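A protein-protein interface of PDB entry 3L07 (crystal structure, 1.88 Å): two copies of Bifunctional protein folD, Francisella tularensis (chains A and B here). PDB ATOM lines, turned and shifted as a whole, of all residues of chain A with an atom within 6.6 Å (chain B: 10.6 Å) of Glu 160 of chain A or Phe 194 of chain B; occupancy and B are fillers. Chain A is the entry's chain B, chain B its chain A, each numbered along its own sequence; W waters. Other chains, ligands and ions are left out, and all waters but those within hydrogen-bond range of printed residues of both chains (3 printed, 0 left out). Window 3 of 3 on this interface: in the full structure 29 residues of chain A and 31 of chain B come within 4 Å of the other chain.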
ATOM      1  N   ARG A 135     -24.424  32.472  -4.503  1.00  0.00           N
ATOM      2  CA  ARG A 135     -24.247  31.768  -5.782  1.00  0.00           C
ATOM      3  C   ARG A 135     -24.929  32.522  -6.911  1.00  0.00           C
ATOM      4  O   ARG A 135     -25.868  32.018  -7.519  1.00  0.00           O
ATOM      5  CB  ARG A 135     -24.834  30.360  -5.664  1.00  0.00           C
ATOM      6  CG  ARG A 135     -23.793  29.249  -5.677  1.00  0.00           C
ATOM      7  CD  ARG A 135     -24.458  27.912  -5.484  1.00  0.00           C
ATOM      8  NE  ARG A 135     -25.049  27.838  -4.144  1.00  0.00           N
ATOM      9  CZ  ARG A 135     -25.382  26.713  -3.513  1.00  0.00           C
ATOM     10  NH1 ARG A 135     -25.876  26.777  -2.282  1.00  0.00           N
ATOM     11  NH2 ARG A 135     -25.201  25.523  -4.084  1.00  0.00           N
ATOM     12  N   ILE A 157      -9.005  17.991  -7.634  1.00  0.00           N
ATOM     13  CA  ILE A 157      -9.285  17.615  -6.269  1.00  0.00           C
ATOM     14  C   ILE A 157     -10.802  17.710  -6.120  1.00  0.00           C
ATOM     15  O   ILE A 157     -11.347  18.770  -6.301  1.00  0.00           O
ATOM     16  CB  ILE A 157      -8.597  18.535  -5.264  1.00  0.00           C
ATOM     17  CG1 ILE A 157      -7.073  18.486  -5.415  1.00  0.00           C
ATOM     18  CG2 ILE A 157      -9.022  18.174  -3.839  1.00  0.00           C
ATOM     19  CD1 ILE A 157      -6.538  17.148  -5.481  1.00  0.00           C
ATOM     20  N   LYS A 158     -11.472  16.585  -5.854  1.00  0.00           N
ATOM     21  CA  LYS A 158     -12.932  16.554  -5.766  1.00  0.00           C
ATOM     22  C   LYS A 158     -13.339  17.322  -4.492  1.00  0.00           C
ATOM     23  O   LYS A 158     -12.738  17.136  -3.429  1.00  0.00           O
ATOM     24  CB  LYS A 158     -13.471  15.088  -5.716  1.00  0.00           C
ATOM     25  CG  LYS A 158     -15.014  14.954  -5.535  1.00  0.00           C
ATOM     26  CD  LYS A 158     -15.474  13.485  -5.316  1.00  0.00           C
ATOM     27  CE  LYS A 158     -16.999  13.327  -5.363  1.00  0.00           C
ATOM     28  NZ  LYS A 158     -17.473  11.911  -5.089  1.00  0.00           N
ATOM     29  N   THR A 159     -14.329  18.195  -4.610  1.00  0.00           N
ATOM     30  CA  THR A 159     -14.895  18.893  -3.428  1.00  0.00           C
ATOM     31  C   THR A 159     -16.212  18.312  -2.971  1.00  0.00           C
ATOM     32  O   THR A 159     -16.540  18.363  -1.794  1.00  0.00           O
ATOM     33  CB  THR A 159     -15.097  20.364  -3.744  1.00  0.00           C
ATOM     34  OG1 THR A 159     -15.900  20.496  -4.940  1.00  0.00           O
ATOM     35  CG2 THR A 159     -13.736  21.004  -3.961  1.00  0.00           C
ATOM     36  N   GLU A 160     -16.980  17.736  -3.884  1.00  0.00           N
ATOM     37  CA  GLU A 160     -18.305  17.230  -3.514  1.00  0.00           C
ATOM     38  C   GLU A 160     -18.246  16.126  -2.491  1.00  0.00           C
ATOM     39  O   GLU A 160     -17.685  15.060  -2.730  1.00  0.00           O
ATOM     40  CB  GLU A 160     -19.129  16.790  -4.739  1.00  0.00           C
ATOM     41  CG  GLU A 160     -20.483  16.098  -4.347  1.00  0.00           C
ATOM     42  CD  GLU A 160     -21.303  15.699  -5.573  1.00  0.00           C
ATOM     43  OE1 GLU A 160     -21.062  16.217  -6.698  1.00  0.00           O
ATOM     44  OE2 GLU A 160     -22.205  14.900  -5.398  1.00  0.00           O
ATOM     45  N   GLY A 161     -18.838  16.387  -1.342  1.00  0.00           N
ATOM     46  CA  GLY A 161     -18.843  15.510  -0.212  1.00  0.00           C
ATOM     47  C   GLY A 161     -17.558  15.471   0.587  1.00  0.00           C
ATOM     48  O   GLY A 161     -17.470  14.741   1.568  1.00  0.00           O
ATOM     49  N   ALA A 162     -16.539  16.217   0.162  1.00  0.00           N
ATOM     50  CA  ALA A 162     -15.304  16.312   0.892  1.00  0.00           C
ATOM     51  C   ALA A 162     -15.527  17.036   2.243  1.00  0.00           C
ATOM     52  O   ALA A 162     -16.422  17.862   2.374  1.00  0.00           O
ATOM     53  CB  ALA A 162     -14.267  17.072   0.038  1.00  0.00           C
ATOM     54  N   ALA A 184     -19.192  24.492  -3.651  1.00  0.00           N
ATOM     55  CA  ALA A 184     -18.652  23.343  -4.385  1.00  0.00           C
ATOM     56  C   ALA A 184     -19.011  21.991  -3.741  1.00  0.00           C
ATOM     57  O   ALA A 184     -18.447  20.928  -4.075  1.00  0.00           O
ATOM     58  CB  ALA A 184     -17.122  23.505  -4.512  1.00  0.00           C
ATOM     59  N   LYS A 185     -19.872  22.067  -2.741  1.00  0.00           N
ATOM     60  CA  LYS A 185     -20.570  20.961  -2.101  1.00  0.00           C
ATOM     61  C   LYS A 185     -19.711  20.201  -1.108  1.00  0.00           C
ATOM     62  O   LYS A 185     -19.966  19.046  -0.770  1.00  0.00           O
ATOM     63  CB  LYS A 185     -21.245  20.014  -3.130  1.00  0.00           C
ATOM     64  CG  LYS A 185     -22.185  20.694  -4.121  1.00  0.00           C
ATOM     65  CD  LYS A 185     -22.679  19.689  -5.207  1.00  0.00           C
ATOM     66  CE  LYS A 185     -23.764  20.342  -6.142  1.00  0.00           C
ATOM     67  NZ  LYS A 185     -23.108  20.927  -7.355  1.00  0.00           N
ATOM     68  N   ALA A 186     -18.650  20.845  -0.638  1.00  0.00           N
ATOM     69  CA  ALA A 186     -17.928  20.311   0.487  1.00  0.00           C
ATOM     70  C   ALA A 186     -18.662  20.629   1.766  1.00  0.00           C
ATOM     71  O   ALA A 186     -19.386  21.605   1.840  1.00  0.00           O
ATOM     72  CB  ALA A 186     -16.488  20.873   0.552  1.00  0.00           C
ATOM     73  N   THR A 187     -18.493  19.771   2.757  1.00  0.00           N
ATOM     74  CA  THR A 187     -18.898  20.059   4.121  1.00  0.00           C
ATOM     75  C   THR A 187     -17.773  20.938   4.708  1.00  0.00           C
ATOM     76  O   THR A 187     -16.597  20.609   4.550  1.00  0.00           O
ATOM     77  CB  THR A 187     -19.004  18.754   4.901  1.00  0.00           C
ATOM     78  OG1 THR A 187     -20.039  17.947   4.291  1.00  0.00           O
ATOM     79  CG2 THR A 187     -19.318  19.054   6.397  1.00  0.00           C
ATOM     80  N   VAL B 166     -24.451  23.458  11.764  1.00  0.00           N
ATOM     81  CA  VAL B 166     -25.606  23.990  11.122  1.00  0.00           C
ATOM     82  C   VAL B 166     -25.959  22.977  10.059  1.00  0.00           C
ATOM     83  O   VAL B 166     -25.171  22.718   9.127  1.00  0.00           O
ATOM     84  CB  VAL B 166     -25.341  25.411  10.509  1.00  0.00           C
ATOM     85  CG1 VAL B 166     -26.587  25.885   9.769  1.00  0.00           C
ATOM     86  CG2 VAL B 166     -25.031  26.383  11.640  1.00  0.00           C
ATOM     87  N   VAL B 167     -27.153  22.411  10.178  1.00  0.00           N
ATOM     88  CA  VAL B 167     -27.625  21.421   9.220  1.00  0.00           C
ATOM     89  C   VAL B 167     -28.610  22.040   8.244  1.00  0.00           C
ATOM     90  O   VAL B 167     -29.743  22.342   8.595  1.00  0.00           O
ATOM     91  CB  VAL B 167     -28.271  20.198   9.899  1.00  0.00           C
ATOM     92  CG1 VAL B 167     -28.555  19.084   8.798  1.00  0.00           C
ATOM     93  CG2 VAL B 167     -27.383  19.668  10.959  1.00  0.00           C
ATOM     94  N   GLY B 168     -28.170  22.223   7.002  1.00  0.00           N
ATOM     95  CA  GLY B 168     -28.926  22.958   6.035  1.00  0.00           C
ATOM     96  C   GLY B 168     -28.085  24.134   5.635  1.00  0.00           C
ATOM     97  O   GLY B 168     -27.586  24.832   6.501  1.00  0.00           O
ATOM     98  N   ALA B 169     -27.863  24.309   4.338  1.00  0.00           N
ATOM     99  CA  ALA B 169     -26.965  25.385   3.874  1.00  0.00           C
ATOM    100  C   ALA B 169     -27.783  26.333   3.031  1.00  0.00           C
ATOM    101  O   ALA B 169     -27.332  26.800   2.023  1.00  0.00           O
ATOM    102  CB  ALA B 169     -25.790  24.782   3.117  1.00  0.00           C
ATOM    103  N   SER B 170     -29.012  26.655   3.453  1.00  0.00           N
ATOM    104  CA  SER B 170     -29.841  27.489   2.641  1.00  0.00           C
ATOM    105  C   SER B 170     -29.397  28.961   2.709  1.00  0.00           C
ATOM    106  O   SER B 170     -28.831  29.412   3.706  1.00  0.00           O
ATOM    107  CB  SER B 170     -31.269  27.399   3.121  1.00  0.00           C
ATOM    108  OG  SER B 170     -31.343  27.951   4.396  1.00  0.00           O
ATOM    109  N   LYS B 175     -26.786  29.462   5.773  1.00  0.00           N
ATOM    110  CA  LYS B 175     -25.567  30.211   5.549  1.00  0.00           C
ATOM    111  C   LYS B 175     -25.491  31.451   6.436  1.00  0.00           C
ATOM    112  O   LYS B 175     -24.496  31.658   7.088  1.00  0.00           O
ATOM    113  CB  LYS B 175     -25.441  30.566   4.082  1.00  0.00           C
ATOM    114  CG  LYS B 175     -25.227  29.374   3.196  1.00  0.00           C
ATOM    115  CD  LYS B 175     -24.875  29.759   1.771  1.00  0.00           C
ATOM    116  CE  LYS B 175     -24.594  28.595   0.880  1.00  0.00           C
ATOM    117  NZ  LYS B 175     -24.610  29.111  -0.551  1.00  0.00           N
ATOM    118  N   THR B 190     -20.868  23.750   8.520  1.00  0.00           N
ATOM    119  CA  THR B 190     -22.088  23.809   7.763  1.00  0.00           C
ATOM    120  C   THR B 190     -22.215  22.500   6.924  1.00  0.00           C
ATOM    121  O   THR B 190     -21.332  22.159   6.096  1.00  0.00           O
ATOM    122  CB  THR B 190     -22.178  25.063   6.890  1.00  0.00           C
ATOM    123  OG1 THR B 190     -22.017  26.251   7.672  1.00  0.00           O
ATOM    124  CG2 THR B 190     -23.551  25.087   6.174  1.00  0.00           C
ATOM    125  N   CYS B 191     -23.303  21.765   7.211  1.00  0.00           N
ATOM    126  CA  CYS B 191     -23.663  20.502   6.533  1.00  0.00           C
ATOM    127  C   CYS B 191     -24.908  20.659   5.637  1.00  0.00           C
ATOM    128  O   CYS B 191     -25.697  21.610   5.780  1.00  0.00           O
ATOM    129  CB  CYS B 191     -23.973  19.425   7.540  1.00  0.00           C
ATOM    130  SG  CYS B 191     -22.726  19.148   8.689  1.00  0.00           S
ATOM    131  N   HIS B 192     -25.054  19.727   4.717  1.00  0.00           N
ATOM    132  CA  HIS B 192     -26.073  19.786   3.694  1.00  0.00           C
ATOM    133  C   HIS B 192     -26.280  18.380   3.089  1.00  0.00           C
ATOM    134  O   HIS B 192     -25.738  17.360   3.586  1.00  0.00           O
ATOM    135  CB  HIS B 192     -25.658  20.829   2.656  1.00  0.00           C
ATOM    136  CG  HIS B 192     -24.230  20.695   2.241  1.00  0.00           C
ATOM    137  ND1 HIS B 192     -23.778  19.642   1.453  1.00  0.00           N
ATOM    138  CD2 HIS B 192     -23.140  21.464   2.516  1.00  0.00           C
ATOM    139  CE1 HIS B 192     -22.470  19.779   1.272  1.00  0.00           C
ATOM    140  NE2 HIS B 192     -22.057  20.865   1.913  1.00  0.00           N
ATOM    141  N   ARG B 193     -27.030  18.331   2.003  1.00  0.00           N
ATOM    142  CA  ARG B 193     -27.434  17.027   1.399  1.00  0.00           C
ATOM    143  C   ARG B 193     -26.276  16.242   0.813  1.00  0.00           C
ATOM    144  O   ARG B 193     -26.413  15.032   0.548  1.00  0.00           O
ATOM    145  CB  ARG B 193     -28.508  17.258   0.345  1.00  0.00           C
ATOM    146  CG  ARG B 193     -28.108  18.004  -0.931  1.00  0.00           C
ATOM    147  CD  ARG B 193     -29.360  18.364  -1.721  1.00  0.00           C
ATOM    148  NE  ARG B 193     -29.059  19.036  -2.992  1.00  0.00           N
ATOM    149  CZ  ARG B 193     -28.950  20.361  -3.184  1.00  0.00           C
ATOM    150  NH1 ARG B 193     -29.078  21.232  -2.184  1.00  0.00           N
ATOM    151  NH2 ARG B 193     -28.692  20.820  -4.408  1.00  0.00           N
ATOM    152  N   PHE B 194     -25.118  16.890   0.621  1.00  0.00           N
ATOM    153  CA  PHE B 194     -23.949  16.178   0.078  1.00  0.00           C
ATOM    154  C   PHE B 194     -22.949  15.761   1.119  1.00  0.00           C
ATOM    155  O   PHE B 194     -21.943  15.112   0.808  1.00  0.00           O
ATOM    156  CB  PHE B 194     -23.275  16.971  -1.012  1.00  0.00           C
ATOM    157  CG  PHE B 194     -24.195  17.399  -2.079  1.00  0.00           C
ATOM    158  CD1 PHE B 194     -24.576  16.513  -3.061  1.00  0.00           C
ATOM    159  CD2 PHE B 194     -24.698  18.678  -2.097  1.00  0.00           C
ATOM    160  CE1 PHE B 194     -25.438  16.906  -4.041  1.00  0.00           C
ATOM    161  CE2 PHE B 194     -25.544  19.087  -3.074  1.00  0.00           C
ATOM    162  CZ  PHE B 194     -25.919  18.195  -4.059  1.00  0.00           C
ATOM    163  N   THR B 195     -23.250  16.084   2.368  1.00  0.00           N
ATOM    164  CA  THR B 195     -22.394  15.759   3.486  1.00  0.00           C
ATOM    165  C   THR B 195     -22.432  14.257   3.684  1.00  0.00           C
ATOM    166  O   THR B 195     -23.533  13.681   3.696  1.00  0.00           O
ATOM    167  CB  THR B 195     -22.912  16.441   4.802  1.00  0.00           C
ATOM    168  OG1 THR B 195     -22.827  17.876   4.694  1.00  0.00           O
ATOM    169  CG2 THR B 195     -22.159  15.980   5.995  1.00  0.00           C
ATOM    170  N   THR B 196     -21.272  13.627   3.832  1.00  0.00           N
ATOM    171  CA  THR B 196     -21.207  12.191   4.122  1.00  0.00           C
ATOM    172  C   THR B 196     -21.048  12.056   5.633  1.00  0.00           C
ATOM    173  O   THR B 196     -20.548  12.946   6.309  1.00  0.00           O
ATOM    174  CB  THR B 196     -20.084  11.497   3.328  1.00  0.00           C
ATOM    175  OG1 THR B 196     -18.842  12.126   3.614  1.00  0.00           O
ATOM    176  CG2 THR B 196     -20.348  11.610   1.840  1.00  0.00           C
ATOM    177  N   ASP B 197     -21.595  10.981   6.166  1.00  0.00           N
ATOM    178  CA  ASP B 197     -21.564  10.729   7.600  1.00  0.00           C
ATOM    179  C   ASP B 197     -21.975  11.955   8.419  1.00  0.00           C
ATOM    180  O   ASP B 197     -21.244  12.417   9.292  1.00  0.00           O
ATOM    181  CB  ASP B 197     -20.187  10.207   8.030  1.00  0.00           C
ATOM    182  CG  ASP B 197     -20.238   9.440   9.348  1.00  0.00           C
ATOM    183  OD1 ASP B 197     -21.307   9.380   9.993  1.00  0.00           O
ATOM    184  OD2 ASP B 197     -19.193   8.884   9.744  1.00  0.00           O
ATOM    185  N   LEU B 198     -23.185  12.433   8.134  1.00  0.00           N
ATOM    186  CA  LEU B 198     -23.761  13.601   8.792  1.00  0.00           C
ATOM    187  C   LEU B 198     -23.653  13.463  10.307  1.00  0.00           C
ATOM    188  O   LEU B 198     -23.229  14.355  10.995  1.00  0.00           O
ATOM    189  CB  LEU B 198     -25.224  13.756   8.355  1.00  0.00           C
ATOM    190  CG  LEU B 198     -26.079  14.936   8.820  1.00  0.00           C
ATOM    191  CD1 LEU B 198     -27.461  14.852   8.204  1.00  0.00           C
ATOM    192  CD2 LEU B 198     -26.196  14.989  10.319  1.00  0.00           C
ATOM    193  N   LYS B 199     -24.035  12.297  10.803  1.00  0.00           N
ATOM    194  CA  LYS B 199     -24.069  12.019  12.223  1.00  0.00           C
ATOM    195  C   LYS B 199     -22.716  12.242  12.939  1.00  0.00           C
ATOM    196  O   LYS B 199     -22.682  12.631  14.107  1.00  0.00           O
ATOM    197  CB  LYS B 199     -24.564  10.566  12.346  1.00  0.00           C
ATOM    198  CG  LYS B 199     -24.623  10.010  13.723  1.00  0.00           C
ATOM    199  CD  LYS B 199     -25.251   8.572  13.738  1.00  0.00           C
ATOM    200  CE  LYS B 199     -24.351   7.494  13.096  1.00  0.00           C
ATOM    201  NZ  LYS B 199     -23.651   6.524  14.029  1.00  0.00           N
ATOM    202  N   HIS B 201     -20.697  14.573  12.512  1.00  0.00           N
ATOM    203  CA  HIS B 201     -20.626  15.975  12.826  1.00  0.00           C
ATOM    204  C   HIS B 201     -21.671  16.327  13.842  1.00  0.00           C
ATOM    205  O   HIS B 201     -21.349  16.879  14.868  1.00  0.00           O
ATOM    206  CB  HIS B 201     -20.855  16.825  11.566  1.00  0.00           C
ATOM    207  CG  HIS B 201     -19.883  16.544  10.476  1.00  0.00           C
ATOM    208  ND1 HIS B 201     -18.557  16.912  10.560  1.00  0.00           N
ATOM    209  CD2 HIS B 201     -20.027  15.899   9.293  1.00  0.00           C
ATOM    210  CE1 HIS B 201     -17.933  16.541   9.451  1.00  0.00           C
ATOM    211  NE2 HIS B 201     -18.796  15.909   8.674  1.00  0.00           N
ATOM    212  N   VAL B 212     -33.640  22.102   7.630  1.00  0.00           N
ATOM    213  CA  VAL B 212     -33.679  21.231   6.448  1.00  0.00           C
ATOM    214  C   VAL B 212     -35.101  21.084   5.882  1.00  0.00           C
ATOM    215  O   VAL B 212     -35.272  20.653   4.750  1.00  0.00           O
ATOM    216  CB  VAL B 212     -33.071  19.868   6.720  1.00  0.00           C
ATOM    217  CG1 VAL B 212     -31.571  19.967   7.044  1.00  0.00           C
ATOM    218  CG2 VAL B 212     -33.788  19.164   7.806  1.00  0.00           C
ATOM    219  N   LYS B 214     -37.541  19.042   6.762  1.00  0.00           N
ATOM    220  CA  LYS B 214     -37.842  17.643   6.713  1.00  0.00           C
ATOM    221  C   LYS B 214     -38.354  17.186   8.098  1.00  0.00           C
ATOM    222  O   LYS B 214     -37.554  17.122   9.043  1.00  0.00           O
ATOM    223  CB  LYS B 214     -36.564  16.857   6.416  1.00  0.00           C
ATOM    224  CG  LYS B 214     -36.130  16.876   4.964  1.00  0.00           C
ATOM    225  CD  LYS B 214     -34.648  16.567   4.862  1.00  0.00           C
ATOM    226  CE  LYS B 214     -34.300  15.799   3.646  1.00  0.00           C
ATOM    227  NZ  LYS B 214     -34.538  14.324   3.908  1.00  0.00           N
ATOM    228  N   PHE B 217     -36.571  14.937  11.083  1.00  0.00           N
ATOM    229  CA  PHE B 217     -35.322  14.487  10.458  1.00  0.00           C
ATOM    230  C   PHE B 217     -34.195  14.144  11.462  1.00  0.00           C
ATOM    231  O   PHE B 217     -33.467  13.182  11.295  1.00  0.00           O
ATOM    232  CB  PHE B 217     -34.833  15.544   9.455  1.00  0.00           C
ATOM    233  CG  PHE B 217     -33.563  15.149   8.751  1.00  0.00           C
ATOM    234  CD1 PHE B 217     -33.565  14.067   7.870  1.00  0.00           C
ATOM    235  CD2 PHE B 217     -32.374  15.800   9.011  1.00  0.00           C
ATOM    236  CE1 PHE B 217     -32.401  13.658   7.242  1.00  0.00           C
ATOM    237  CE2 PHE B 217     -31.196  15.400   8.398  1.00  0.00           C
ATOM    238  CZ  PHE B 217     -31.214  14.318   7.497  1.00  0.00           C
HETATM  239  O   HOH W   1     -27.701  27.160  -0.562  1.00  0.00           O
HETATM  240  O   HOH W   2     -16.894  12.322   2.065  1.00  0.00           O
HETATM  241  O   HOH W   3     -18.974  15.568   3.803  1.00  0.00           O
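The guanidinium group (NH1) of Arg 135 of chain A lies close to the side-chain amino group (NZ) of Lys 175 of chain B.
NE2 of His 192 of chain B sits at hydrogen-bond distance from O of Ala 186 of chain A.
The side-chain hydroxyl (OG1) of Thr 187 of chain A is in hydrogen-bond range of the side-chain hydroxyl (OG1) of Thr 195 of chain B, 2.8 Å away.
No position is printed for both chains.
Of the 11 pairs that touch across the chains among the printed residues, none has its exchanged pair printed and touching as well.
The backbone NH (N) of His 192 of chain B sits at hydrogen-bond distance from the side-chain hydroxyl (OG1) of Thr 195 of chain B, at 2.9 Å.
The backbone carbonyl oxygen of Thr 159 of chain A sits close to the backbone NH of Ala 186 of chain A (3.5 Å).
The backbone carbonyl oxygen (O) of Ser 170 of chain B is in hydrogen-bond range of the backbone NH (N) of Lys 175 of chain B, 2.9 Å away.
N of Phe 194 of chain B lies close to ND1 of His 192 of chain B.
N of Thr 187 of chain A sits at hydrogen-bond distance from O of Ala 162 of chain A, 2.8 Å away.
The backbone carbonyl oxygen (O) of Lys 185 of chain A is in hydrogen-bond range of the backbone NH (N) of Gly 161 of chain A (2.9 Å).
Phe 194 of chain B touches Glu 160 of chain A (CD1 to OE2, 3.7 Å).
Phe 194 of chain B touches Gly 161 of chain A.
Gly 161 of chain A touches Thr 196 of chain B (O to OG1, 3.6 Å).
His 192 of chain B touches Lys 185 of chain A.
Phe 194 of chain B touches Lys 185 of chain A.
Thr 187 of chain A touches Thr 190 of chain B (CG2 to O, 3.7 Å).
NE2 of His 192 of chain B touches N of Thr 187 of chain A (3.8 Å).
CG2 of Thr 187 of chain A touches NE2 of His 201 of chain B, 3.9 Å away.
Water W2 bridges the side-chain hydroxyl of Thr 196 of chain B (2.5 Å) and the backbone carbonyl oxygen of Gly 161 of chain A (2.5 Å).
Water W1 bridges the guanidinium group of Arg 135 of chain A (2.5 Å) and the backbone carbonyl oxygen of Ala 169 of chain B (2.6 Å).
Water W3 lies within hydrogen-bond range of OG1 of Thr 187 of chain A, O of Gly 161 of chain A and N of Thr 196 of chain B.
Of the 20 printed residues of chain B, 7 touch a printed residue of chain A.
Of the 11 printed residues of chain A, 6 touch a printed residue of chain B.
Of the printed residues of chain B, Arg 135 of chain A touches Lys 175 (3.2 Å).
Ile 157 of chain A touches none of the printed residues of chain B.
Thr 159 of chain A touches none of the printed residues of chain B.
Glu 160 of chain A touches just one residue of chain B: Phe 194 (3.7 Å).
No residue of chain B comes within 4 Å of Ala 162 of chain A.
Lys 185 of chain A touches just these residues of chain B: His 192 and Phe 194.
Of the printed residues of chain A, Lys 175 of chain B touches Arg 135.
Printed residues of chain A within 4 Å of Thr 190 of chain B: Thr 187 (3.7 Å).
Phe 194 of chain B touches just these residues of chain A: Glu 160, Gly 161 and Lys 185.
Lys 199 of chain B touches none of the printed residues of chain A.
The nearest residue of chain B that does not touch Glu 160 of chain A is Thr 196 of chain B (6.3 Å).
The nearest residue of chain A that does not touch Phe 194 of chain B is Thr 187 of chain A (4.8 Å).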
